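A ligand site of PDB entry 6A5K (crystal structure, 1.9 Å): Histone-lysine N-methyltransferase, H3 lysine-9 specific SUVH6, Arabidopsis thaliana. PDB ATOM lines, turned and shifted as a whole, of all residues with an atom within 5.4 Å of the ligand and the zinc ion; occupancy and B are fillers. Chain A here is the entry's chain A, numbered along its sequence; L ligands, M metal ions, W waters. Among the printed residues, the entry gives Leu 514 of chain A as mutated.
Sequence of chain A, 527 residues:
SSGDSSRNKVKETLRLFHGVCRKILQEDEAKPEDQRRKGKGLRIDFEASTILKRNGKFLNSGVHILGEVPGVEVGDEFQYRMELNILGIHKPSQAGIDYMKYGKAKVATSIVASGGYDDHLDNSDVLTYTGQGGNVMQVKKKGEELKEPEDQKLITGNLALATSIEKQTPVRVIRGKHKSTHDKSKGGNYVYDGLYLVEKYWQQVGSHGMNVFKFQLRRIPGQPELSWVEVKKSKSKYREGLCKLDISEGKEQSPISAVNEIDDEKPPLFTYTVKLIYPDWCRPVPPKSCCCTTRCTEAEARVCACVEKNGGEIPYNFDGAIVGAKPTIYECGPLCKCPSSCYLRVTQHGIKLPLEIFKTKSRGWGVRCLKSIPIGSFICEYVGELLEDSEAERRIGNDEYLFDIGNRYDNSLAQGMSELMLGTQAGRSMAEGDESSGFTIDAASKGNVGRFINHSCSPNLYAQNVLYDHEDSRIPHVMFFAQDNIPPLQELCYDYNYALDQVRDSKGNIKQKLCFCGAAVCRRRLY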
ATOM      1  N   PRO A 268       3.168  26.500  35.369  1.00  0.00           N
ATOM      2  CA  PRO A 268       3.449  25.205  35.985  1.00  0.00           C
ATOM      3  C   PRO A 268       4.872  24.718  35.737  1.00  0.00           C
ATOM      4  O   PRO A 268       5.548  25.152  34.813  1.00  0.00           O
ATOM      5  CB  PRO A 268       2.434  24.275  35.335  1.00  0.00           C
ATOM      6  CG  PRO A 268       2.143  24.908  34.016  1.00  0.00           C
ATOM      7  CD  PRO A 268       2.188  26.385  34.274  1.00  0.00           C
ATOM      8  N   SER A 362     -11.201  29.624  33.013  1.00  0.00           N
ATOM      9  CA  SER A 362     -11.743  28.299  33.278  1.00  0.00           C
ATOM     10  C   SER A 362     -10.941  27.124  32.697  1.00  0.00           C
ATOM     11  O   SER A 362     -11.275  25.965  32.964  1.00  0.00           O
ATOM     12  CB  SER A 362     -13.194  28.227  32.774  1.00  0.00           C
ATOM     13  OG  SER A 362     -13.270  28.281  31.362  1.00  0.00           O
ATOM     14  N   ARG A 363      -9.884  27.404  31.938  1.00  0.00           N
ATOM     15  CA  ARG A 363      -9.142  26.326  31.281  1.00  0.00           C
ATOM     16  C   ARG A 363      -7.638  26.387  31.572  1.00  0.00           C
ATOM     17  O   ARG A 363      -6.837  25.895  30.785  1.00  0.00           O
ATOM     18  CB  ARG A 363      -9.374  26.372  29.762  1.00  0.00           C
ATOM     19  CG  ARG A 363     -10.796  26.010  29.369  1.00  0.00           C
ATOM     20  CD  ARG A 363     -11.064  26.254  27.867  1.00  0.00           C
ATOM     21  NE  ARG A 363     -10.568  27.560  27.429  1.00  0.00           N
ATOM     22  CZ  ARG A 363     -11.094  28.729  27.769  1.00  0.00           C
ATOM     23  NH1 ARG A 363     -12.162  28.767  28.549  1.00  0.00           N
ATOM     24  NH2 ARG A 363     -10.546  29.859  27.338  1.00  0.00           N
ATOM     25  N   GLY A 364      -7.282  26.956  32.718  1.00  0.00           N
ATOM     26  CA  GLY A 364      -5.874  27.087  33.100  1.00  0.00           C
ATOM     27  C   GLY A 364      -5.083  27.954  32.141  1.00  0.00           C
ATOM     28  O   GLY A 364      -5.546  28.991  31.681  1.00  0.00           O
ATOM     29  N   TRP A 365      -3.864  27.520  31.834  1.00  0.00           N
ATOM     30  CA  TRP A 365      -3.007  28.252  30.912  1.00  0.00           C
ATOM     31  C   TRP A 365      -3.317  27.880  29.460  1.00  0.00           C
ATOM     32  O   TRP A 365      -3.614  26.721  29.167  1.00  0.00           O
ATOM     33  CB  TRP A 365      -1.537  27.990  31.230  1.00  0.00           C
ATOM     34  CG  TRP A 365      -1.127  28.495  32.576  1.00  0.00           C
ATOM     35  CD1 TRP A 365      -1.250  27.844  33.773  1.00  0.00           C
ATOM     36  CD2 TRP A 365      -0.549  29.780  32.875  1.00  0.00           C
ATOM     37  NE1 TRP A 365      -0.777  28.634  34.798  1.00  0.00           N
ATOM     38  CE2 TRP A 365      -0.345  29.825  34.273  1.00  0.00           C
ATOM     39  CE3 TRP A 365      -0.194  30.880  32.098  1.00  0.00           C
ATOM     40  CZ2 TRP A 365       0.216  30.938  34.906  1.00  0.00           C
ATOM     41  CZ3 TRP A 365       0.364  31.979  32.728  1.00  0.00           C
ATOM     42  CH2 TRP A 365       0.556  32.001  34.112  1.00  0.00           C
ATOM     43  N   GLY A 366      -3.257  28.870  28.583  1.00  0.00           N
ATOM     44  CA  GLY A 366      -3.401  28.671  27.146  1.00  0.00           C
ATOM     45  C   GLY A 366      -2.338  29.428  26.368  1.00  0.00           C
ATOM     46  O   GLY A 366      -1.434  30.016  26.962  1.00  0.00           O
ATOM     47  N   TYR A 382       4.224  20.042  18.378  1.00  0.00           N
ATOM     48  CA  TYR A 382       3.980  19.434  19.682  1.00  0.00           C
ATOM     49  C   TYR A 382       5.208  18.627  20.067  1.00  0.00           C
ATOM     50  O   TYR A 382       5.423  17.527  19.567  1.00  0.00           O
ATOM     51  CB  TYR A 382       2.727  18.540  19.680  1.00  0.00           C
ATOM     52  CG  TYR A 382       2.246  18.226  21.076  1.00  0.00           C
ATOM     53  CD1 TYR A 382       2.795  17.177  21.806  1.00  0.00           C
ATOM     54  CD2 TYR A 382       1.235  18.974  21.661  1.00  0.00           C
ATOM     55  CE1 TYR A 382       2.360  16.899  23.092  1.00  0.00           C
ATOM     56  CE2 TYR A 382       0.791  18.706  22.944  1.00  0.00           C
ATOM     57  CZ  TYR A 382       1.360  17.658  23.652  1.00  0.00           C
ATOM     58  OH  TYR A 382       0.919  17.382  24.929  1.00  0.00           O
ATOM     59  N   ASP A 399      -1.407  12.421  31.945  1.00  0.00           N
ATOM     60  CA  ASP A 399      -2.578  12.249  31.081  1.00  0.00           C
ATOM     61  C   ASP A 399      -3.029  13.547  30.430  1.00  0.00           C
ATOM     62  O   ASP A 399      -3.626  13.522  29.366  1.00  0.00           O
ATOM     63  CB  ASP A 399      -3.747  11.642  31.862  1.00  0.00           C
ATOM     64  CG  ASP A 399      -4.440  12.648  32.767  1.00  0.00           C
ATOM     65  OD1 ASP A 399      -4.128  12.672  33.977  1.00  0.00           O
ATOM     66  OD2 ASP A 399      -5.304  13.407  32.280  1.00  0.00           O
ATOM     67  N   GLU A 400      -2.736  14.685  31.066  1.00  0.00           N
ATOM     68  CA  GLU A 400      -3.181  15.966  30.525  1.00  0.00           C
ATOM     69  C   GLU A 400      -2.258  16.515  29.454  1.00  0.00           C
ATOM     70  O   GLU A 400      -2.567  17.534  28.841  1.00  0.00           O
ATOM     71  CB  GLU A 400      -3.350  16.987  31.655  1.00  0.00           C
ATOM     72  CG  GLU A 400      -4.566  16.719  32.532  1.00  0.00           C
ATOM     73  CD  GLU A 400      -4.855  17.858  33.482  1.00  0.00           C
ATOM     74  OE1 GLU A 400      -4.016  18.140  34.366  1.00  0.00           O
ATOM     75  OE2 GLU A 400      -5.923  18.486  33.341  1.00  0.00           O
ATOM     76  N   TYR A 401      -1.145  15.836  29.194  1.00  0.00           N
ATOM     77  CA  TYR A 401      -0.164  16.338  28.242  1.00  0.00           C
ATOM     78  C   TYR A 401       0.267  15.281  27.239  1.00  0.00           C
ATOM     79  O   TYR A 401       1.439  15.192  26.863  1.00  0.00           O
ATOM     80  CB  TYR A 401       1.052  16.903  28.988  1.00  0.00           C
ATOM     81  CG  TYR A 401       0.672  18.043  29.895  1.00  0.00           C
ATOM     82  CD1 TYR A 401       0.393  19.303  29.373  1.00  0.00           C
ATOM     83  CD2 TYR A 401       0.540  17.860  31.271  1.00  0.00           C
ATOM     84  CE1 TYR A 401       0.020  20.356  30.197  1.00  0.00           C
ATOM     85  CE2 TYR A 401       0.164  18.899  32.092  1.00  0.00           C
ATOM     86  CZ  TYR A 401      -0.086  20.149  31.551  1.00  0.00           C
ATOM     87  OH  TYR A 401      -0.462  21.188  32.372  1.00  0.00           O
ATOM     88  N   ARG A 451       2.428  22.126  24.584  1.00  0.00           N
ATOM     89  CA  ARG A 451       1.724  21.461  25.683  1.00  0.00           C
ATOM     90  C   ARG A 451       0.624  22.355  26.274  1.00  0.00           C
ATOM     91  O   ARG A 451      -0.255  21.883  26.975  1.00  0.00           O
ATOM     92  CB  ARG A 451       2.699  21.032  26.796  1.00  0.00           C
ATOM     93  CG  ARG A 451       3.170  22.185  27.685  1.00  0.00           C
ATOM     94  CD  ARG A 451       4.428  21.852  28.493  1.00  0.00           C
ATOM     95  NE  ARG A 451       4.223  20.789  29.486  1.00  0.00           N
ATOM     96  CZ  ARG A 451       3.603  20.959  30.647  1.00  0.00           C
ATOM     97  NH1 ARG A 451       3.092  22.136  30.970  1.00  0.00           N
ATOM     98  NH2 ARG A 451       3.466  19.936  31.484  1.00  0.00           N
ATOM     99  N   PHE A 452       0.668  23.659  25.993  1.00  0.00           N
ATOM    100  CA  PHE A 452      -0.264  24.592  26.635  1.00  0.00           C
ATOM    101  C   PHE A 452      -1.457  24.953  25.765  1.00  0.00           C
ATOM    102  O   PHE A 452      -2.371  25.652  26.231  1.00  0.00           O
ATOM    103  CB  PHE A 452       0.471  25.867  27.047  1.00  0.00           C
ATOM    104  CG  PHE A 452       1.363  25.700  28.237  1.00  0.00           C
ATOM    105  CD1 PHE A 452       2.740  25.786  28.105  1.00  0.00           C
ATOM    106  CD2 PHE A 452       0.825  25.459  29.497  1.00  0.00           C
ATOM    107  CE1 PHE A 452       3.573  25.644  29.205  1.00  0.00           C
ATOM    108  CE2 PHE A 452       1.650  25.311  30.600  1.00  0.00           C
ATOM    109  CZ  PHE A 452       3.027  25.392  30.454  1.00  0.00           C
ATOM    110  N   ILE A 453      -1.482  24.492  24.518  1.00  0.00           N
ATOM    111  CA  ILE A 453      -2.599  24.813  23.615  1.00  0.00           C
ATOM    112  C   ILE A 453      -3.870  24.056  24.030  1.00  0.00           C
ATOM    113  O   ILE A 453      -3.866  22.820  24.116  1.00  0.00           O
ATOM    114  CB  ILE A 453      -2.267  24.481  22.140  1.00  0.00           C
ATOM    115  CG1 ILE A 453      -1.006  25.239  21.694  1.00  0.00           C
ATOM    116  CG2 ILE A 453      -3.445  24.841  21.225  1.00  0.00           C
ATOM    117  CD1 ILE A 453      -0.478  24.790  20.345  1.00  0.00           C
ATOM    118  N   ASN A 454      -4.934  24.794  24.307  1.00  0.00           N
ATOM    119  CA  ASN A 454      -6.183  24.216  24.796  1.00  0.00           C
ATOM    120  C   ASN A 454      -7.054  23.644  23.674  1.00  0.00           C
ATOM    121  O   ASN A 454      -6.801  23.865  22.507  1.00  0.00           O
ATOM    122  CB  ASN A 454      -6.962  25.258  25.593  1.00  0.00           C
ATOM    123  CG  ASN A 454      -6.384  25.486  26.977  1.00  0.00           C
ATOM    124  OD1 ASN A 454      -5.869  24.557  27.600  1.00  0.00           O
ATOM    125  ND2 ASN A 454      -6.450  26.724  27.465  1.00  0.00           N
ATOM    126  N   HIS A 455      -8.080  22.902  24.065  1.00  0.00           N
ATOM    127  CA  HIS A 455      -9.042  22.368  23.103  1.00  0.00           C
ATOM    128  C   HIS A 455     -10.156  23.370  22.793  1.00  0.00           C
ATOM    129  O   HIS A 455     -10.599  24.107  23.679  1.00  0.00           O
ATOM    130  CB  HIS A 455      -9.683  21.078  23.627  1.00  0.00           C
ATOM    131  CG  HIS A 455     -10.956  20.726  22.915  1.00  0.00           C
ATOM    132  ND1 HIS A 455     -10.967  20.026  21.733  1.00  0.00           N
ATOM    133  CD2 HIS A 455     -12.250  21.019  23.203  1.00  0.00           C
ATOM    134  CE1 HIS A 455     -12.222  19.874  21.319  1.00  0.00           C
ATOM    135  NE2 HIS A 455     -13.016  20.471  22.198  1.00  0.00           N
ATOM    136  N   SER A 456     -10.610  23.365  21.549  1.00  0.00           N
ATOM    137  CA  SER A 456     -11.855  24.046  21.213  1.00  0.00           C
ATOM    138  C   SER A 456     -12.701  23.230  20.232  1.00  0.00           C
ATOM    139  O   SER A 456     -12.162  22.543  19.357  1.00  0.00           O
ATOM    140  CB  SER A 456     -11.585  25.431  20.618  1.00  0.00           C
ATOM    141  OG  SER A 456     -12.808  26.085  20.284  1.00  0.00           O
ATOM    142  N   CYS A 457     -14.013  23.317  20.388  1.00  0.00           N
ATOM    143  CA  CYS A 457     -14.939  22.671  19.463  1.00  0.00           C
ATOM    144  C   CYS A 457     -15.088  23.505  18.194  1.00  0.00           C
ATOM    145  O   CYS A 457     -15.648  23.048  17.200  1.00  0.00           O
ATOM    146  CB  CYS A 457     -16.291  22.445  20.119  1.00  0.00           C
ATOM    147  SG  CYS A 457     -16.205  21.384  21.584  1.00  0.00           S
ATOM    148  N   TYR A 496      -8.892  18.401  20.342  1.00  0.00           N
ATOM    149  CA  TYR A 496      -8.217  17.329  21.079  1.00  0.00           C
ATOM    150  C   TYR A 496      -8.638  15.938  20.619  1.00  0.00           C
ATOM    151  O   TYR A 496      -7.894  14.963  20.762  1.00  0.00           O
ATOM    152  CB  TYR A 496      -8.477  17.431  22.577  1.00  0.00           C
ATOM    153  CG  TYR A 496      -7.574  18.372  23.329  1.00  0.00           C
ATOM    154  CD1 TYR A 496      -6.809  19.330  22.669  1.00  0.00           C
ATOM    155  CD2 TYR A 496      -7.493  18.306  24.722  1.00  0.00           C
ATOM    156  CE1 TYR A 496      -5.979  20.200  23.378  1.00  0.00           C
ATOM    157  CE2 TYR A 496      -6.671  19.171  25.434  1.00  0.00           C
ATOM    158  CZ  TYR A 496      -5.922  20.112  24.764  1.00  0.00           C
ATOM    159  OH  TYR A 496      -5.106  20.958  25.497  1.00  0.00           O
ATOM    160  N   LYS A 513     -15.301  14.997  31.935  1.00  0.00           N
ATOM    161  CA  LYS A 513     -14.882  16.374  32.116  1.00  0.00           C
ATOM    162  C   LYS A 513     -15.610  17.255  31.116  1.00  0.00           C
ATOM    163  O   LYS A 513     -15.668  16.943  29.939  1.00  0.00           O
ATOM    164  CB  LYS A 513     -13.359  16.513  31.956  1.00  0.00           C
ATOM    165  CG  LYS A 513     -12.883  17.953  32.055  1.00  0.00           C
ATOM    166  CD  LYS A 513     -11.386  18.025  32.306  1.00  0.00           C
ATOM    167  CE  LYS A 513     -10.928  19.469  32.404  1.00  0.00           C
ATOM    168  NZ  LYS A 513     -11.507  20.168  33.582  1.00  0.00           N
ATOM    169  N   LEU A 514     -16.177  18.350  31.609  1.00  0.00           N
ATOM    170  CA  LEU A 514     -16.917  19.269  30.761  1.00  0.00           C
ATOM    171  C   LEU A 514     -15.974  20.070  29.874  1.00  0.00           C
ATOM    172  O   LEU A 514     -14.850  20.382  30.274  1.00  0.00           O
ATOM    173  CB  LEU A 514     -17.772  20.212  31.615  1.00  0.00           C
ATOM    174  CG  LEU A 514     -18.893  19.592  32.436  1.00  0.00           C
ATOM    175  CD1 LEU A 514     -19.498  20.614  33.416  1.00  0.00           C
ATOM    176  CD2 LEU A 514     -19.982  19.040  31.527  1.00  0.00           C
ATOM    177  N   CYS A 515     -16.420  20.396  28.668  1.00  0.00           N
ATOM    178  CA  CYS A 515     -15.684  21.300  27.802  1.00  0.00           C
ATOM    179  C   CYS A 515     -16.069  22.741  28.108  1.00  0.00           C
ATOM    180  O   CYS A 515     -17.259  23.072  28.135  1.00  0.00           O
ATOM    181  CB  CYS A 515     -15.936  20.988  26.314  1.00  0.00           C
ATOM    182  SG  CYS A 515     -14.990  22.052  25.205  1.00  0.00           S
ATOM    183  N   PHE A 516     -15.070  23.587  28.331  1.00  0.00           N
ATOM    184  CA  PHE A 516     -15.289  24.999  28.630  1.00  0.00           C
ATOM    185  C   PHE A 516     -14.815  25.904  27.492  1.00  0.00           C
ATOM    186  O   PHE A 516     -14.438  27.056  27.726  1.00  0.00           O
ATOM    187  CB  PHE A 516     -14.559  25.382  29.922  1.00  0.00           C
ATOM    188  CG  PHE A 516     -15.177  24.791  31.166  1.00  0.00           C
ATOM    189  CD1 PHE A 516     -16.494  24.361  31.182  1.00  0.00           C
ATOM    190  CD2 PHE A 516     -14.425  24.677  32.334  1.00  0.00           C
ATOM    191  CE1 PHE A 516     -17.060  23.833  32.322  1.00  0.00           C
ATOM    192  CE2 PHE A 516     -14.986  24.146  33.483  1.00  0.00           C
ATOM    193  CZ  PHE A 516     -16.308  23.714  33.476  1.00  0.00           C
ATOM    194  N   CYS A 517     -14.835  25.394  26.261  1.00  0.00           N
ATOM    195  CA  CYS A 517     -14.293  26.169  25.135  1.00  0.00           C
ATOM    196  C   CYS A 517     -15.159  27.407  24.838  1.00  0.00           C
ATOM    197  O   CYS A 517     -14.657  28.396  24.313  1.00  0.00           O
ATOM    198  CB  CYS A 517     -14.167  25.300  23.865  1.00  0.00           C
ATOM    199  SG  CYS A 517     -15.707  24.986  22.920  1.00  0.00           S
ATOM    200  N   GLY A 518     -16.441  27.328  25.183  1.00  0.00           N
ATOM    201  CA  GLY A 518     -17.342  28.466  25.040  1.00  0.00           C
ATOM    202  C   GLY A 518     -17.923  28.700  23.651  1.00  0.00           C
ATOM    203  O   GLY A 518     -18.635  29.687  23.421  1.00  0.00           O
ATOM    204  N   ALA A 519     -17.632  27.793  22.719  1.00  0.00           N
ATOM    205  CA  ALA A 519     -18.185  27.892  21.375  1.00  0.00           C
ATOM    206  C   ALA A 519     -19.688  27.625  21.384  1.00  0.00           C
ATOM    207  O   ALA A 519     -20.205  26.898  22.225  1.00  0.00           O
ATOM    208  CB  ALA A 519     -17.484  26.929  20.433  1.00  0.00           C
ATOM    209  N   CYS A 522     -20.435  23.919  20.869  1.00  0.00           N
ATOM    210  CA  CYS A 522     -19.684  23.063  21.793  1.00  0.00           C
ATOM    211  C   CYS A 522     -20.303  21.671  21.970  1.00  0.00           C
ATOM    212  O   CYS A 522     -21.515  21.531  22.111  1.00  0.00           O
ATOM    213  CB  CYS A 522     -19.562  23.753  23.148  1.00  0.00           C
ATOM    214  SG  CYS A 522     -18.590  22.861  24.379  1.00  0.00           S
ATOM    215  N   ARG A 523     -19.459  20.646  21.957  1.00  0.00           N
ATOM    216  CA  ARG A 523     -19.912  19.275  22.133  1.00  0.00           C
ATOM    217  C   ARG A 523     -19.974  18.897  23.618  1.00  0.00           C
ATOM    218  O   ARG A 523     -20.232  17.738  23.972  1.00  0.00           O
ATOM    219  CB  ARG A 523     -19.003  18.346  21.326  1.00  0.00           C
ATOM    220  CG  ARG A 523     -18.939  18.810  19.857  1.00  0.00           C
ATOM    221  CD  ARG A 523     -18.293  17.811  18.898  1.00  0.00           C
ATOM    222  NE  ARG A 523     -16.839  17.848  18.945  1.00  0.00           N
ATOM    223  CZ  ARG A 523     -16.085  18.778  18.353  1.00  0.00           C
ATOM    224  NH1 ARG A 523     -16.636  19.760  17.660  1.00  0.00           N
ATOM    225  NH2 ARG A 523     -14.763  18.706  18.461  1.00  0.00           N
ATOM    226  N   ARG A 524     -19.731  19.891  24.459  1.00  0.00           N
ATOM    227  CA  ARG A 524     -20.089  19.896  25.895  1.00  0.00           C
ATOM    228  C   ARG A 524     -19.177  19.080  26.803  1.00  0.00           C
ATOM    229  O   ARG A 524     -19.011  19.420  27.976  1.00  0.00           O
ATOM    230  CB  ARG A 524     -21.540  19.430  26.081  1.00  0.00           C
ATOM    231  CG  ARG A 524     -22.589  20.308  25.416  1.00  0.00           C
ATOM    232  CD  ARG A 524     -22.349  21.796  25.652  1.00  0.00           C
ATOM    233  NE  ARG A 524     -22.405  22.172  27.071  1.00  0.00           N
ATOM    234  CZ  ARG A 524     -23.542  22.342  27.755  1.00  0.00           C
ATOM    235  NH1 ARG A 524     -24.709  22.163  27.163  1.00  0.00           N
ATOM    236  NH2 ARG A 524     -23.494  22.687  29.034  1.00  0.00           N
ATOM    237  N   LEU A 526     -15.250  17.324  27.262  1.00  0.00           N
ATOM    238  CA  LEU A 526     -13.873  17.172  26.784  1.00  0.00           C
ATOM    239  C   LEU A 526     -13.567  15.676  26.646  1.00  0.00           C
ATOM    240  O   LEU A 526     -12.917  15.247  25.691  1.00  0.00           O
ATOM    241  CB  LEU A 526     -12.894  17.849  27.750  1.00  0.00           C
ATOM    242  CG  LEU A 526     -11.444  18.019  27.282  1.00  0.00           C
ATOM    243  CD1 LEU A 526     -11.357  18.896  26.040  1.00  0.00           C
ATOM    244  CD2 LEU A 526     -10.589  18.595  28.404  1.00  0.00           C
HETATM  245  N1  LIG L   1      -4.712  24.410  30.241  1.00  0.00           N
HETATM  246  C1  LIG L   1      -3.509  23.571  30.354  1.00  0.00           C
HETATM  247  C2  LIG L   1      -2.534  24.047  31.433  1.00  0.00           C
HETATM  248  O1  LIG L   1      -1.421  23.518  31.548  1.00  0.00           O
HETATM  249  O2  LIG L   1      -2.833  24.969  32.195  1.00  0.00           O
HETATM  250  C3  LIG L   1      -2.785  23.483  29.008  1.00  0.00           C
HETATM  251  C4  LIG L   1      -3.474  22.493  28.082  1.00  0.00           C
HETATM  252  S1  LIG L   1      -3.247  20.831  28.769  1.00  0.00           S
HETATM  253  C5  LIG L   1      -2.486  20.052  27.355  1.00  0.00           C
HETATM  254  C6  LIG L   1      -4.867  20.056  28.644  1.00  0.00           C
HETATM  255  C7  LIG L   1      -5.719  20.388  29.859  1.00  0.00           C
HETATM  256  O3  LIG L   1      -6.203  21.725  29.755  1.00  0.00           O
HETATM  257  C8  LIG L   1      -6.935  19.491  29.933  1.00  0.00           C
HETATM  258  O4  LIG L   1      -6.667  18.321  30.671  1.00  0.00           O
HETATM  259  C9  LIG L   1      -7.919  20.383  30.649  1.00  0.00           C
HETATM  260  O5  LIG L   1      -7.620  20.351  32.027  1.00  0.00           O
HETATM  261  C10 LIG L   1      -7.555  21.764  30.143  1.00  0.00           C
HETATM  262  N2  LIG L   1      -8.386  22.106  28.968  1.00  0.00           N
HETATM  263  C11 LIG L   1      -7.970  22.308  27.678  1.00  0.00           C
HETATM  264  N3  LIG L   1      -9.050  22.599  26.912  1.00  0.00           N
HETATM  265  C12 LIG L   1     -10.162  22.558  27.689  1.00  0.00           C
HETATM  266  C13 LIG L   1     -11.505  22.769  27.438  1.00  0.00           C
HETATM  267  N4  LIG L   1     -11.938  23.069  26.203  1.00  0.00           N
HETATM  268  N5  LIG L   1     -12.415  22.644  28.456  1.00  0.00           N
HETATM  269  C14 LIG L   1     -11.995  22.330  29.740  1.00  0.00           C
HETATM  270  N6  LIG L   1     -10.649  22.132  29.994  1.00  0.00           N
HETATM  271  C15 LIG L   1      -9.746  22.255  28.992  1.00  0.00           C
HETATM  272 ZN    ZN M   1     -16.456  22.823  23.515  1.00  0.00          ZN
HETATM  273  O   HOH W   1     -10.430  22.838  32.894  1.00  0.00           O
HETATM  274  O   HOH W   2      -5.771  23.385  32.817  1.00  0.00           O
HETATM  275  O   HOH W   3      -2.946  24.521  35.061  1.00  0.00           O
HETATM  276  O   HOH W   4      -6.552  16.317  28.752  1.00  0.00           O
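A nitrogen (N5) of the ligand is in hydrogen-bond range of the backbone NH of Phe 516, at 2.8 Å.
OH of Tyr 401 lies within hydrogen-bond range of O1 of the ligand.
O of Trp 365 lies within hydrogen-bond range of N1 of the ligand, 2.8 Å away.
The side-chain sulfur (SG) of Cys 515 sits close to a nitrogen (N4) of the ligand, at 3.4 Å.
O2 of the ligand lies within hydrogen-bond range of N of Trp 365, 2.8 Å away.
N4 of the ligand is in hydrogen-bond range of O of His 455, at 3.0 Å.
The backbone carbonyl oxygen (O) of Arg 363 lies within hydrogen-bond range of a nitrogen (N1) of the ligand, 2.6 Å away.
An oxygen (O4) of the ligand lies within hydrogen-bond range of the side-chain carboxylate (OE2) of Glu 400.
A nitrogen (N3) of the ligand sits at hydrogen-bond distance from the backbone NH (N) of His 455, 3.0 Å away.
A nitrogen (N1) of the ligand is in hydrogen-bond range of the side-chain amide oxygen (OD1) of Asn 454.
The backbone NH (N) of Leu 526 lies within hydrogen-bond range of the backbone carbonyl oxygen (O) of Lys 513 (2.7 Å).
The backbone carbonyl oxygen of Arg 524 lies within hydrogen-bond range of the backbone NH of Cys 515 (2.9 Å).
The side-chain sulfur (SG) of Cys 457 lies close to a ring nitrogen (NE2) of His 455 (3.4 Å).
The backbone carbonyl oxygen (O) of Trp 365 sits at hydrogen-bond distance from the side-chain amide nitrogen (ND2) of Asn 454, 3.3 Å away.
A ring nitrogen (ND1) of His 455 sits at hydrogen-bond distance from the backbone NH (N) of Tyr 496, 3.0 Å away.
NH1 of Arg 523 is in hydrogen-bond range of O of Cys 457 (3.5 Å).
The side-chain amide nitrogen of Asn 454 sits at hydrogen-bond distance from the backbone carbonyl oxygen of Arg 363.
The backbone NH (N) of Ala 519 sits close to the side-chain sulfur (SG) of Cys 517 (3.4 Å).
A sulfur (S1) of the ligand sits close to the backbone carbonyl oxygen of Arg 451 (3.6 Å).
The side-chain hydroxyl of Tyr 496 sits close to a sulfur (S1) of the ligand, 3.8 Å away.
Merely in contact with the ligand: Gly 364 (3.7 Å), Phe 452 (3.5 Å), Ile 453 (3.999 Å), Lys 513 (3.4 Å), Leu 514 (3.5 Å) and Leu 526 (3.8 Å).
Hydrophobic or aromatic side chains that line the ligand: Trp 365, Tyr 401, Phe 452, His 455, Tyr 496, Phe 516 and Leu 526.
The nearest printed residue that does not touch the ligand is Pro 268 (4.6 Å).
Within 4 Å of the zinc ion: Cys 457, Cys 515, Cys 517 and Cys 522.
The nearest printed residue that does not touch the zinc ion is Arg 523 (4.02 Å).
The zinc ion is bound by SG of Cys 522, SG of Cys 517, SG of Cys 515 and SG of Cys 457.
The zinc ion has four donor atoms within binding distance.
Water W2 bridges N1 of the ligand (3.0 Å) and O of Arg 363 (3.4 Å).
Water W1 lies within hydrogen-bond range of the side-chain amino group of Lys 513, a nitrogen (N6) of the ligand and the backbone carbonyl oxygen of Ser 362.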
